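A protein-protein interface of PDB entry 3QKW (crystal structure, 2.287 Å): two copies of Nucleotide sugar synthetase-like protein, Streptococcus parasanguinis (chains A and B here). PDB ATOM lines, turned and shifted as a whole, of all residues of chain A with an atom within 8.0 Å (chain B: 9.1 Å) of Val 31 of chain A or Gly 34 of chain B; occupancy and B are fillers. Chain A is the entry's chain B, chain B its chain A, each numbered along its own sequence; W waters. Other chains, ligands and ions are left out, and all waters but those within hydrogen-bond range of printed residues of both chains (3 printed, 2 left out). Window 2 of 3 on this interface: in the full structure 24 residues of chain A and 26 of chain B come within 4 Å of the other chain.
Gly 34 of chain B touches Val 31 of chain A (O to CG1, 3.95 Å). NE of Arg 36 of chain B touches CG2 of Val 31 of chain A, at 3.9 Å. Thr 27 of chain B touches Arg 36 of chain A (CG2 to NH1, 3.9 Å). Arg 36 of chain A touches Val 31 of chain B (NE to CG2, 3.97 Å).
The side-chain hydroxyl of Tyr 6 of chain B is in hydrogen-bond range of the side-chain carboxylate of Glu 37 of chain A. The side-chain carboxylate (OD1) of Asp 28 of chain B is in salt-bridge range of the guanidinium group (NH2) of Arg 36 of chain A (2.7 Å). The guanidinium group (NH1) of Arg 36 of chain B is in salt-bridge range of the side-chain carboxylate (OE1) of Glu 37 of chain A, 3.0 Å away. The side-chain carboxylate of Asp 28 of chain A is in salt-bridge range of the guanidinium group of Arg 36 of chain B (2.7 Å). The guanidinium group (NH1) of Arg 36 of chain A lies within salt-bridge range of the side-chain carboxylate (OE1) of Glu 37 of chain B (3.0 Å).
The backbone carbonyl oxygen (O) of Arg 36 of chain B lies within hydrogen-bond range of the backbone NH (N) of Ile 7 of chain B (2.8 Å). O of Arg 36 of chain A sits at hydrogen-bond distance from N of Ile 7 of chain A, at 2.7 Å. The backbone carbonyl oxygen of Val 5 of chain B lies within hydrogen-bond range of the backbone NH of Arg 36 of chain B (2.8 Å). The side-chain carboxylate of Glu 37 of chain A is in hydrogen-bond range of the side-chain amide nitrogen of Asn 9 of chain A.
Asp 28 of chain A touches Arg 36 of chain B, and with the chains exchanged Arg 36 of chain A touches Asp 28 of chain B. Val 31 of chain A touches Gly 34 of chain B, but with the chains exchanged Gly 34 of chain A does not touch Val 31 of chain B (4.03 Å). Val 31 of chain A touches Arg 36 of chain B, and with the chains exchanged Arg 36 of chain A touches Val 31 of chain B. Arg 36 of chain A touches Glu 37 of chain B, and with the chains exchanged Glu 37 of chain A touches Arg 36 of chain B.
Hydrophobic or aromatic side chains of chain B that line the printed part of chain A: Tyr 6 and Val 31. Among the printed residues, 9 pairs touch across the chains. Among the printed residues, Asp or Glu carboxylates within 4 Å of a Lys or Arg side-chain nitrogen of the other chain: Asp 28 of chain A with Arg 36 of chain B (2.7 Å), Arg 36 of chain A with Asp 28 of chain B (2.7 Å), Arg 36 of chain A with Glu 37 of chain B (3.0 Å) and Glu 37 of chain A with Arg 36 of chain B (3.0 Å).
Val 31 of chain A touches just these residues of chain B: Gly 34 (3.95 Å) and Arg 36 (3.9 Å). Gly 34 of chain B touches just one residue of chain A: Val 31. No residue of chain B comes within 4 Å of Ala 30 of chain A. Of the printed residues of chain A, Glu 37 of chain B touches Arg 36 (3.0 Å). Of the printed residues of chain A, Val 31 of chain B touches Arg 36 (3.97 Å). Printed residues of chain A within 4 Å of Thr 27 of chain B: Arg 36 (3.9 Å). Leu 322 of chain B touches none of the printed residues of chain A. Gly 34 of chain A touches none of the printed residues of chain B. The nearest residue of chain B that does not touch Val 31 of chain A is Tyr 35 of chain B (4.8 Å). The nearest residue of chain A that does not touch Gly 34 of chain B is Ser 32 of chain A (6.7 Å).
Water W2 bridges NH1 of Arg 36 of chain A (2.9 Å) and OD1 of Asp 28 of chain B (3.1 Å). Water W1 lies within hydrogen-bond range of the side-chain carboxylate (OE1) of Glu 37 of chain A, the guanidinium group (NH1) of Arg 4 of chain B and the side-chain hydroxyl (OH) of Tyr 6 of chain B.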
ATOM      1  N   VAL A   5     -19.908 -35.247   3.160  1.00  0.00           N
ATOM      2  CA  VAL A   5     -19.609 -34.627   1.873  1.00  0.00           C
ATOM      3  C   VAL A   5     -19.357 -33.121   2.074  1.00  0.00           C
ATOM      4  O   VAL A   5     -20.162 -32.438   2.698  1.00  0.00           O
ATOM      5  CB  VAL A   5     -20.791 -34.792   0.891  1.00  0.00           C
ATOM      6  CG1 VAL A   5     -20.556 -34.003  -0.351  1.00  0.00           C
ATOM      7  CG2 VAL A   5     -21.035 -36.243   0.569  1.00  0.00           C
ATOM      8  N   ILE A   7     -18.293 -29.191   0.236  1.00  0.00           N
ATOM      9  CA  ILE A   7     -18.234 -28.451  -1.009  1.00  0.00           C
ATOM     10  C   ILE A   7     -17.633 -27.070  -0.786  1.00  0.00           C
ATOM     11  O   ILE A   7     -18.007 -26.368   0.152  1.00  0.00           O
ATOM     12  CB  ILE A   7     -19.622 -28.328  -1.656  1.00  0.00           C
ATOM     13  CG1 ILE A   7     -19.555 -27.512  -2.949  1.00  0.00           C
ATOM     14  CG2 ILE A   7     -20.592 -27.707  -0.677  1.00  0.00           C
ATOM     15  CD1 ILE A   7     -20.801 -27.684  -3.831  1.00  0.00           C
ATOM     16  N   ASN A   9     -16.930 -23.150  -1.395  1.00  0.00           N
ATOM     17  CA  ASN A   9     -17.805 -22.046  -1.733  1.00  0.00           C
ATOM     18  C   ASN A   9     -17.121 -20.681  -1.566  1.00  0.00           C
ATOM     19  O   ASN A   9     -16.763 -20.308  -0.455  1.00  0.00           O
ATOM     20  CB  ASN A   9     -18.998 -22.098  -0.797  1.00  0.00           C
ATOM     21  CG  ASN A   9     -20.087 -21.150  -1.199  1.00  0.00           C
ATOM     22  OD1 ASN A   9     -20.256 -20.853  -2.382  1.00  0.00           O
ATOM     23  ND2 ASN A   9     -20.843 -20.666  -0.217  1.00  0.00           N
ATOM     24  N   ASN A  24     -22.565 -19.934  -4.668  1.00  0.00           N
ATOM     25  CA  ASN A  24     -23.429 -19.801  -3.498  1.00  0.00           C
ATOM     26  C   ASN A  24     -24.764 -20.513  -3.684  1.00  0.00           C
ATOM     27  O   ASN A  24     -25.295 -21.103  -2.737  1.00  0.00           O
ATOM     28  CB  ASN A  24     -23.703 -18.327  -3.192  1.00  0.00           C
ATOM     29  CG  ASN A  24     -22.486 -17.602  -2.700  1.00  0.00           C
ATOM     30  OD1 ASN A  24     -22.474 -16.371  -2.603  1.00  0.00           O
ATOM     31  ND2 ASN A  24     -21.447 -18.354  -2.391  1.00  0.00           N
ATOM     32  N   THR A  25     -25.309 -20.441  -4.899  1.00  0.00           N
ATOM     33  CA  THR A  25     -26.555 -21.149  -5.217  1.00  0.00           C
ATOM     34  C   THR A  25     -26.355 -22.663  -5.119  1.00  0.00           C
ATOM     35  O   THR A  25     -27.118 -23.352  -4.448  1.00  0.00           O
ATOM     36  CB  THR A  25     -27.105 -20.773  -6.611  1.00  0.00           C
ATOM     37  OG1 THR A  25     -27.515 -19.407  -6.596  1.00  0.00           O
ATOM     38  CG2 THR A  25     -28.321 -21.631  -6.952  1.00  0.00           C
ATOM     39  N   VAL A  26     -25.312 -23.171  -5.772  1.00  0.00           N
ATOM     40  CA  VAL A  26     -24.963 -24.584  -5.639  1.00  0.00           C
ATOM     41  C   VAL A  26     -24.789 -24.971  -4.177  1.00  0.00           C
ATOM     42  O   VAL A  26     -25.299 -26.018  -3.730  1.00  0.00           O
ATOM     43  CB  VAL A  26     -23.696 -24.942  -6.422  1.00  0.00           C
ATOM     44  CG1 VAL A  26     -23.370 -26.422  -6.247  1.00  0.00           C
ATOM     45  CG2 VAL A  26     -23.892 -24.613  -7.874  1.00  0.00           C
ATOM     46  N   THR A  27     -24.095 -24.124  -3.416  1.00  0.00           N
ATOM     47  CA  THR A  27     -23.825 -24.446  -2.012  1.00  0.00           C
ATOM     48  C   THR A  27     -25.100 -24.537  -1.146  1.00  0.00           C
ATOM     49  O   THR A  27     -25.253 -25.477  -0.352  1.00  0.00           O
ATOM     50  CB  THR A  27     -22.759 -23.526  -1.398  1.00  0.00           C
ATOM     51  OG1 THR A  27     -21.554 -23.633  -2.168  1.00  0.00           O
ATOM     52  CG2 THR A  27     -22.466 -23.937   0.039  1.00  0.00           C
ATOM     53  N   ASP A  28     -26.018 -23.592  -1.332  1.00  0.00           N
ATOM     54  CA  ASP A  28     -27.307 -23.607  -0.628  1.00  0.00           C
ATOM     55  C   ASP A  28     -28.105 -24.903  -0.905  1.00  0.00           C
ATOM     56  O   ASP A  28     -28.700 -25.482  -0.007  1.00  0.00           O
ATOM     57  CB  ASP A  28     -28.168 -22.395  -1.019  1.00  0.00           C
ATOM     58  CG  ASP A  28     -27.568 -21.054  -0.571  1.00  0.00           C
ATOM     59  OD1 ASP A  28     -26.682 -21.020   0.315  1.00  0.00           O
ATOM     60  OD2 ASP A  28     -28.012 -20.013  -1.107  1.00  0.00           O
ATOM     61  N   VAL A  29     -28.130 -25.328  -2.161  1.00  0.00           N
ATOM     62  CA  VAL A  29     -28.672 -26.630  -2.515  1.00  0.00           C
ATOM     63  C   VAL A  29     -27.904 -27.741  -1.785  1.00  0.00           C
ATOM     64  O   VAL A  29     -28.503 -28.578  -1.111  1.00  0.00           O
ATOM     65  CB  VAL A  29     -28.616 -26.842  -4.023  1.00  0.00           C
ATOM     66  CG1 VAL A  29     -29.143 -28.228  -4.393  1.00  0.00           C
ATOM     67  CG2 VAL A  29     -29.436 -25.773  -4.704  1.00  0.00           C
ATOM     68  N   ALA A  30     -26.578 -27.709  -1.873  1.00  0.00           N
ATOM     69  CA  ALA A  30     -25.753 -28.715  -1.203  1.00  0.00           C
ATOM     70  C   ALA A  30     -26.094 -28.816   0.278  1.00  0.00           C
ATOM     71  O   ALA A  30     -26.193 -29.924   0.823  1.00  0.00           O
ATOM     72  CB  ALA A  30     -24.269 -28.447  -1.411  1.00  0.00           C
ATOM     73  N   VAL A  31     -26.288 -27.673   0.929  1.00  0.00           N
ATOM     74  CA  VAL A  31     -26.629 -27.671   2.345  1.00  0.00           C
ATOM     75  C   VAL A  31     -28.000 -28.301   2.597  1.00  0.00           C
ATOM     76  O   VAL A  31     -28.183 -29.023   3.581  1.00  0.00           O
ATOM     77  CB  VAL A  31     -26.606 -26.262   2.951  1.00  0.00           C
ATOM     78  CG1 VAL A  31     -27.085 -26.316   4.391  1.00  0.00           C
ATOM     79  CG2 VAL A  31     -25.207 -25.683   2.882  1.00  0.00           C
ATOM     80  N   SER A  32     -28.969 -28.026   1.723  1.00  0.00           N
ATOM     81  CA  SER A  32     -30.280 -28.639   1.883  1.00  0.00           C
ATOM     82  C   SER A  32     -30.163 -30.162   1.772  1.00  0.00           C
ATOM     83  O   SER A  32     -30.907 -30.870   2.427  1.00  0.00           O
ATOM     84  CB  SER A  32     -31.321 -28.075   0.899  1.00  0.00           C
ATOM     85  OG  SER A  32     -31.042 -28.444  -0.433  1.00  0.00           O
ATOM     86  N   LEU A  33     -29.206 -30.642   0.969  1.00  0.00           N
ATOM     87  CA  LEU A  33     -28.911 -32.068   0.847  1.00  0.00           C
ATOM     88  C   LEU A  33     -28.057 -32.635   1.995  1.00  0.00           C
ATOM     89  O   LEU A  33     -27.785 -33.841   2.054  1.00  0.00           O
ATOM     90  CB  LEU A  33     -28.231 -32.381  -0.483  1.00  0.00           C
ATOM     91  CG  LEU A  33     -29.003 -32.012  -1.747  1.00  0.00           C
ATOM     92  CD1 LEU A  33     -28.214 -32.390  -3.005  1.00  0.00           C
ATOM     93  CD2 LEU A  33     -30.381 -32.678  -1.748  1.00  0.00           C
ATOM     94  N   GLY A  34     -27.653 -31.777   2.921  1.00  0.00           N
ATOM     95  CA  GLY A  34     -26.867 -32.222   4.057  1.00  0.00           C
ATOM     96  C   GLY A  34     -25.353 -32.122   3.878  1.00  0.00           C
ATOM     97  O   GLY A  34     -24.605 -32.545   4.758  1.00  0.00           O
ATOM     98  N   TYR A  35     -24.899 -31.567   2.753  1.00  0.00           N
ATOM     99  CA  TYR A  35     -23.463 -31.403   2.499  1.00  0.00           C
ATOM    100  C   TYR A  35     -22.928 -30.222   3.313  1.00  0.00           C
ATOM    101  O   TYR A  35     -23.699 -29.354   3.713  1.00  0.00           O
ATOM    102  CB  TYR A  35     -23.192 -31.149   1.012  1.00  0.00           C
ATOM    103  CG  TYR A  35     -23.569 -32.279   0.075  1.00  0.00           C
ATOM    104  CD1 TYR A  35     -24.259 -33.414   0.535  1.00  0.00           C
ATOM    105  CD2 TYR A  35     -23.245 -32.209  -1.281  1.00  0.00           C
ATOM    106  CE1 TYR A  35     -24.620 -34.441  -0.334  1.00  0.00           C
ATOM    107  CE2 TYR A  35     -23.575 -33.227  -2.150  1.00  0.00           C
ATOM    108  CZ  TYR A  35     -24.268 -34.343  -1.674  1.00  0.00           C
ATOM    109  OH  TYR A  35     -24.598 -35.342  -2.547  1.00  0.00           O
ATOM    110  N   ARG A  36     -21.613 -30.181   3.539  1.00  0.00           N
ATOM    111  CA  ARG A  36     -21.007 -29.143   4.370  1.00  0.00           C
ATOM    112  C   ARG A  36     -20.151 -28.161   3.556  1.00  0.00           C
ATOM    113  O   ARG A  36     -19.409 -28.548   2.644  1.00  0.00           O
ATOM    114  CB  ARG A  36     -20.197 -29.779   5.518  1.00  0.00           C
ATOM    115  CG  ARG A  36     -21.021 -30.764   6.380  1.00  0.00           C
ATOM    116  CD  ARG A  36     -20.267 -31.315   7.607  1.00  0.00           C
ATOM    117  NE  ARG A  36     -21.134 -32.186   8.409  1.00  0.00           N
ATOM    118  CZ  ARG A  36     -20.957 -32.487   9.693  1.00  0.00           C
ATOM    119  NH1 ARG A  36     -19.922 -31.992  10.363  1.00  0.00           N
ATOM    120  NH2 ARG A  36     -21.816 -33.295  10.316  1.00  0.00           N
ATOM    121  N   GLU A  37     -20.257 -26.881   3.885  1.00  0.00           N
ATOM    122  CA  GLU A  37     -19.478 -25.860   3.194  1.00  0.00           C
ATOM    123  C   GLU A  37     -18.006 -25.824   3.617  1.00  0.00           C
ATOM    124  O   GLU A  37     -17.714 -25.835   4.797  1.00  0.00           O
ATOM    125  CB  GLU A  37     -20.065 -24.495   3.485  1.00  0.00           C
ATOM    126  CG  GLU A  37     -19.206 -23.352   2.988  1.00  0.00           C
ATOM    127  CD  GLU A  37     -19.717 -22.017   3.473  1.00  0.00           C
ATOM    128  OE1 GLU A  37     -20.456 -21.353   2.717  1.00  0.00           O
ATOM    129  OE2 GLU A  37     -19.418 -21.651   4.628  1.00  0.00           O
ATOM    130  N   ARG A 319     -29.337 -30.634  -7.860  1.00  0.00           N
ATOM    131  CA  ARG A 319     -29.526 -31.757  -6.959  1.00  0.00           C
ATOM    132  C   ARG A 319     -29.004 -33.034  -7.611  1.00  0.00           C
ATOM    133  O   ARG A 319     -28.331 -33.832  -6.969  1.00  0.00           O
ATOM    134  CB  ARG A 319     -30.989 -31.894  -6.514  1.00  0.00           C
ATOM    135  CG  ARG A 319     -31.407 -30.898  -5.441  1.00  0.00           C
ATOM    136  CD  ARG A 319     -32.915 -30.875  -5.278  1.00  0.00           C
ATOM    137  NE  ARG A 319     -33.382 -31.996  -4.477  1.00  0.00           N
ATOM    138  CZ  ARG A 319     -33.678 -31.907  -3.184  1.00  0.00           C
ATOM    139  NH1 ARG A 319     -33.568 -30.740  -2.543  1.00  0.00           N
ATOM    140  NH2 ARG A 319     -34.091 -32.985  -2.535  1.00  0.00           N
ATOM    141  N   LEU A 322     -25.071 -33.076  -7.877  1.00  0.00           N
ATOM    142  CA  LEU A 322     -24.489 -33.187  -6.542  1.00  0.00           C
ATOM    143  C   LEU A 322     -24.670 -34.615  -5.991  1.00  0.00           C
ATOM    144  O   LEU A 322     -23.910 -35.090  -5.141  1.00  0.00           O
ATOM    145  CB  LEU A 322     -25.179 -32.184  -5.607  1.00  0.00           C
ATOM    146  CG  LEU A 322     -24.510 -30.899  -5.099  1.00  0.00           C
ATOM    147  CD1 LEU A 322     -23.299 -30.445  -5.904  1.00  0.00           C
ATOM    148  CD2 LEU A 322     -25.550 -29.813  -5.010  1.00  0.00           C
ATOM    149  N   MET B   3     -29.514 -14.286   6.354  1.00  0.00           N
ATOM    150  CA  MET B   3     -28.813 -14.840   7.508  1.00  0.00           C
ATOM    151  C   MET B   3     -28.500 -16.349   7.406  1.00  0.00           C
ATOM    152  O   MET B   3     -29.345 -17.122   6.976  1.00  0.00           O
ATOM    153  CB  MET B   3     -29.627 -14.578   8.777  1.00  0.00           C
ATOM    154  CG  MET B   3     -29.249 -15.503   9.920  1.00  0.00           C
ATOM    155  SD  MET B   3     -30.241 -15.230  11.395  1.00  0.00           S
ATOM    156  CE  MET B   3     -29.913 -13.482  11.674  1.00  0.00           C
ATOM    157  N   ARG B   4     -27.280 -16.747   7.782  1.00  0.00           N
ATOM    158  CA  ARG B   4     -26.948 -18.162   7.988  1.00  0.00           C
ATOM    159  C   ARG B   4     -26.503 -18.356   9.424  1.00  0.00           C
ATOM    160  O   ARG B   4     -26.008 -17.434  10.064  1.00  0.00           O
ATOM    161  CB  ARG B   4     -25.844 -18.656   7.049  1.00  0.00           C
ATOM    162  CG  ARG B   4     -26.219 -18.775   5.577  1.00  0.00           C
ATOM    163  CD  ARG B   4     -26.104 -17.425   4.898  1.00  0.00           C
ATOM    164  NE  ARG B   4     -24.845 -16.783   5.261  1.00  0.00           N
ATOM    165  CZ  ARG B   4     -23.695 -16.975   4.622  1.00  0.00           C
ATOM    166  NH1 ARG B   4     -23.630 -17.783   3.570  1.00  0.00           N
ATOM    167  NH2 ARG B   4     -22.608 -16.356   5.037  1.00  0.00           N
ATOM    168  N   VAL B   5     -26.684 -19.555   9.939  1.00  0.00           N
ATOM    169  CA  VAL B   5     -26.172 -19.875  11.258  1.00  0.00           C
ATOM    170  C   VAL B   5     -24.957 -20.799  11.119  1.00  0.00           C
ATOM    171  O   VAL B   5     -25.009 -21.806  10.425  1.00  0.00           O
ATOM    172  CB  VAL B   5     -27.240 -20.552  12.136  1.00  0.00           C
ATOM    173  CG1 VAL B   5     -26.686 -20.819  13.528  1.00  0.00           C
ATOM    174  CG2 VAL B   5     -28.464 -19.680  12.226  1.00  0.00           C
ATOM    175  N   TYR B   6     -23.863 -20.451  11.776  1.00  0.00           N
ATOM    176  CA  TYR B   6     -22.682 -21.287  11.746  1.00  0.00           C
ATOM    177  C   TYR B   6     -22.441 -21.789  13.146  1.00  0.00           C
ATOM    178  O   TYR B   6     -22.884 -21.163  14.107  1.00  0.00           O
ATOM    179  CB  TYR B   6     -21.479 -20.478  11.258  1.00  0.00           C
ATOM    180  CG  TYR B   6     -21.365 -20.314   9.754  1.00  0.00           C
ATOM    181  CD1 TYR B   6     -22.153 -19.392   9.071  1.00  0.00           C
ATOM    182  CD2 TYR B   6     -20.436 -21.053   9.024  1.00  0.00           C
ATOM    183  CE1 TYR B   6     -22.029 -19.217   7.700  1.00  0.00           C
ATOM    184  CE2 TYR B   6     -20.309 -20.893   7.655  1.00  0.00           C
ATOM    185  CZ  TYR B   6     -21.103 -19.969   7.000  1.00  0.00           C
ATOM    186  OH  TYR B   6     -20.994 -19.812   5.639  1.00  0.00           O
ATOM    187  N   ILE B   7     -21.753 -22.925  13.261  1.00  0.00           N
ATOM    188  CA  ILE B   7     -21.365 -23.448  14.563  1.00  0.00           C
ATOM    189  C   ILE B   7     -19.953 -24.038  14.542  1.00  0.00           C
ATOM    190  O   ILE B   7     -19.610 -24.813  13.647  1.00  0.00           O
ATOM    191  CB  ILE B   7     -22.366 -24.485  15.062  1.00  0.00           C
ATOM    192  CG1 ILE B   7     -21.909 -25.055  16.396  1.00  0.00           C
ATOM    193  CG2 ILE B   7     -22.583 -25.591  14.021  1.00  0.00           C
ATOM    194  CD1 ILE B   7     -23.032 -25.716  17.144  1.00  0.00           C
ATOM    195  N   THR B  27     -22.993 -30.672  16.415  1.00  0.00           N
ATOM    196  CA  THR B  27     -22.799 -30.196  15.048  1.00  0.00           C
ATOM    197  C   THR B  27     -23.660 -30.967  14.070  1.00  0.00           C
ATOM    198  O   THR B  27     -24.276 -30.367  13.197  1.00  0.00           O
ATOM    199  CB  THR B  27     -21.303 -30.234  14.626  1.00  0.00           C
ATOM    200  OG1 THR B  27     -20.540 -29.479  15.571  1.00  0.00           O
ATOM    201  CG2 THR B  27     -21.104 -29.612  13.243  1.00  0.00           C
ATOM    202  N   ASP B  28     -23.711 -32.288  14.228  1.00  0.00           N
ATOM    203  CA  ASP B  28     -24.592 -33.134  13.419  1.00  0.00           C
ATOM    204  C   ASP B  28     -26.069 -32.704  13.538  1.00  0.00           C
ATOM    205  O   ASP B  28     -26.767 -32.595  12.536  1.00  0.00           O
ATOM    206  CB  ASP B  28     -24.461 -34.613  13.823  1.00  0.00           C
ATOM    207  CG  ASP B  28     -23.112 -35.247  13.407  1.00  0.00           C
ATOM    208  OD1 ASP B  28     -22.327 -34.607  12.654  1.00  0.00           O
ATOM    209  OD2 ASP B  28     -22.852 -36.403  13.837  1.00  0.00           O
ATOM    210  N   VAL B  29     -26.539 -32.475  14.759  1.00  0.00           N
ATOM    211  CA  VAL B  29     -27.907 -31.992  14.957  1.00  0.00           C
ATOM    212  C   VAL B  29     -28.046 -30.660  14.228  1.00  0.00           C
ATOM    213  O   VAL B  29     -28.964 -30.466  13.425  1.00  0.00           O
ATOM    214  CB  VAL B  29     -28.233 -31.811  16.442  1.00  0.00           C
ATOM    215  CG1 VAL B  29     -29.645 -31.253  16.620  1.00  0.00           C
ATOM    216  CG2 VAL B  29     -28.090 -33.141  17.182  1.00  0.00           C
ATOM    217  N   ALA B  30     -27.102 -29.761  14.490  1.00  0.00           N
ATOM    218  CA  ALA B  30     -27.073 -28.456  13.844  1.00  0.00           C
ATOM    219  C   ALA B  30     -27.161 -28.547  12.327  1.00  0.00           C
ATOM    220  O   ALA B  30     -27.904 -27.813  11.704  1.00  0.00           O
ATOM    221  CB  ALA B  30     -25.828 -27.677  14.255  1.00  0.00           C
ATOM    222  N   VAL B  31     -26.399 -29.445  11.726  1.00  0.00           N
ATOM    223  CA  VAL B  31     -26.422 -29.558  10.273  1.00  0.00           C
ATOM    224  C   VAL B  31     -27.810 -30.029   9.773  1.00  0.00           C
ATOM    225  O   VAL B  31     -28.254 -29.638   8.701  1.00  0.00           O
ATOM    226  CB  VAL B  31     -25.316 -30.518   9.798  1.00  0.00           C
ATOM    227  CG1 VAL B  31     -25.511 -30.906   8.325  1.00  0.00           C
ATOM    228  CG2 VAL B  31     -23.948 -29.899  10.022  1.00  0.00           C
ATOM    229  N   SER B  32     -28.489 -30.872  10.555  1.00  0.00           N
ATOM    230  CA  SER B  32     -29.805 -31.353  10.167  1.00  0.00           C
ATOM    231  C   SER B  32     -30.814 -30.218  10.272  1.00  0.00           C
ATOM    232  O   SER B  32     -31.848 -30.256   9.624  1.00  0.00           O
ATOM    233  CB  SER B  32     -30.241 -32.543  11.032  1.00  0.00           C
ATOM    234  OG  SER B  32     -30.707 -32.098  12.288  1.00  0.00           O
ATOM    235  N   LEU B  33     -30.495 -29.210  11.086  1.00  0.00           N
ATOM    236  CA  LEU B  33     -31.294 -27.989  11.184  1.00  0.00           C
ATOM    237  C   LEU B  33     -30.885 -26.951  10.128  1.00  0.00           C
ATOM    238  O   LEU B  33     -31.415 -25.842  10.110  1.00  0.00           O
ATOM    239  CB  LEU B  33     -31.186 -27.364  12.582  1.00  0.00           C
ATOM    240  CG  LEU B  33     -31.652 -28.179  13.798  1.00  0.00           C
ATOM    241  CD1 LEU B  33     -31.441 -27.419  15.102  1.00  0.00           C
ATOM    242  CD2 LEU B  33     -33.119 -28.602  13.669  1.00  0.00           C
ATOM    243  N   GLY B  34     -29.944 -27.299   9.251  1.00  0.00           N
ATOM    244  CA  GLY B  34     -29.476 -26.367   8.228  1.00  0.00           C
ATOM    245  C   GLY B  34     -28.344 -25.427   8.617  1.00  0.00           C
ATOM    246  O   GLY B  34     -27.943 -24.556   7.825  1.00  0.00           O
ATOM    247  N   TYR B  35     -27.813 -25.588   9.824  1.00  0.00           N
ATOM    248  CA  TYR B  35     -26.678 -24.774  10.244  1.00  0.00           C
ATOM    249  C   TYR B  35     -25.411 -25.198   9.496  1.00  0.00           C
ATOM    250  O   TYR B  35     -25.356 -26.260   8.881  1.00  0.00           O
ATOM    251  CB  TYR B  35     -26.446 -24.877  11.754  1.00  0.00           C
ATOM    252  CG  TYR B  35     -27.540 -24.306  12.634  1.00  0.00           C
ATOM    253  CD1 TYR B  35     -28.789 -23.953  12.115  1.00  0.00           C
ATOM    254  CD2 TYR B  35     -27.331 -24.141  13.998  1.00  0.00           C
ATOM    255  CE1 TYR B  35     -29.794 -23.444  12.939  1.00  0.00           C
ATOM    256  CE2 TYR B  35     -28.314 -23.628  14.829  1.00  0.00           C
ATOM    257  CZ  TYR B  35     -29.550 -23.281  14.292  1.00  0.00           C
ATOM    258  OH  TYR B  35     -30.529 -22.775  15.124  1.00  0.00           O
ATOM    259  N   ARG B  36     -24.388 -24.363   9.568  1.00  0.00           N
ATOM    260  CA  ARG B  36     -23.154 -24.605   8.827  1.00  0.00           C
ATOM    261  C   ARG B  36     -21.953 -24.745   9.763  1.00  0.00           C
ATOM    262  O   ARG B  36     -21.758 -23.946  10.674  1.00  0.00           O
ATOM    263  CB  ARG B  36     -22.908 -23.473   7.828  1.00  0.00           C
ATOM    264  CG  ARG B  36     -24.049 -23.236   6.858  1.00  0.00           C
ATOM    265  CD  ARG B  36     -23.611 -22.431   5.639  1.00  0.00           C
ATOM    266  NE  ARG B  36     -24.726 -22.256   4.717  1.00  0.00           N
ATOM    267  CZ  ARG B  36     -24.615 -21.780   3.483  1.00  0.00           C
ATOM    268  NH1 ARG B  36     -23.434 -21.416   3.004  1.00  0.00           N
ATOM    269  NH2 ARG B  36     -25.696 -21.653   2.726  1.00  0.00           N
ATOM    270  N   GLU B  37     -21.151 -25.766   9.522  1.00  0.00           N
ATOM    271  CA  GLU B  37     -19.962 -26.024  10.323  1.00  0.00           C
ATOM    272  C   GLU B  37     -18.794 -25.069  10.043  1.00  0.00           C
ATOM    273  O   GLU B  37     -18.424 -24.843   8.887  1.00  0.00           O
ATOM    274  CB  GLU B  37     -19.485 -27.476  10.135  1.00  0.00           C
ATOM    275  CG  GLU B  37     -18.105 -27.759  10.758  1.00  0.00           C
ATOM    276  CD  GLU B  37     -17.530 -29.099  10.334  1.00  0.00           C
ATOM    277  OE1 GLU B  37     -17.733 -30.082  11.059  1.00  0.00           O
ATOM    278  OE2 GLU B  37     -16.875 -29.172   9.282  1.00  0.00           O
ATOM    279  N   ARG B 319     -31.612 -29.804  19.944  1.00  0.00           N
ATOM    280  CA  ARG B 319     -32.435 -29.064  18.985  1.00  0.00           C
ATOM    281  C   ARG B 319     -33.054 -27.826  19.606  1.00  0.00           C
ATOM    282  O   ARG B 319     -33.084 -26.780  18.969  1.00  0.00           O
ATOM    283  CB  ARG B 319     -33.519 -29.926  18.358  1.00  0.00           C
ATOM    284  CG  ARG B 319     -33.023 -30.962  17.406  1.00  0.00           C
ATOM    285  CD  ARG B 319     -34.089 -31.988  17.209  1.00  0.00           C
ATOM    286  NE  ARG B 319     -35.090 -31.482  16.297  1.00  0.00           N
ATOM    287  CZ  ARG B 319     -35.034 -31.649  14.982  1.00  0.00           C
ATOM    288  NH1 ARG B 319     -34.010 -32.324  14.439  1.00  0.00           N
ATOM    289  NH2 ARG B 319     -36.010 -31.147  14.225  1.00  0.00           N
ATOM    290  N   LEU B 322     -30.243 -25.189  20.353  1.00  0.00           N
ATOM    291  CA  LEU B 322     -29.754 -24.624  19.102  1.00  0.00           C
ATOM    292  C   LEU B 322     -30.785 -23.674  18.490  1.00  0.00           C
ATOM    293  O   LEU B 322     -30.427 -22.702  17.816  1.00  0.00           O
ATOM    294  CB  LEU B 322     -29.447 -25.729  18.097  1.00  0.00           C
ATOM    295  CG  LEU B 322     -28.011 -26.209  17.851  1.00  0.00           C
ATOM    296  CD1 LEU B 322     -27.043 -25.806  18.945  1.00  0.00           C
ATOM    297  CD2 LEU B 322     -28.000 -27.715  17.617  1.00  0.00           C
HETATM  298  O   HOH W   1     -20.753 -18.380   2.677  1.00  0.00           O
HETATM  299  O   HOH W   2     -19.583 -33.243  12.993  1.00  0.00           O
HETATM  300  O   HOH W   3     -23.791 -20.587   0.239  1.00  0.00           O
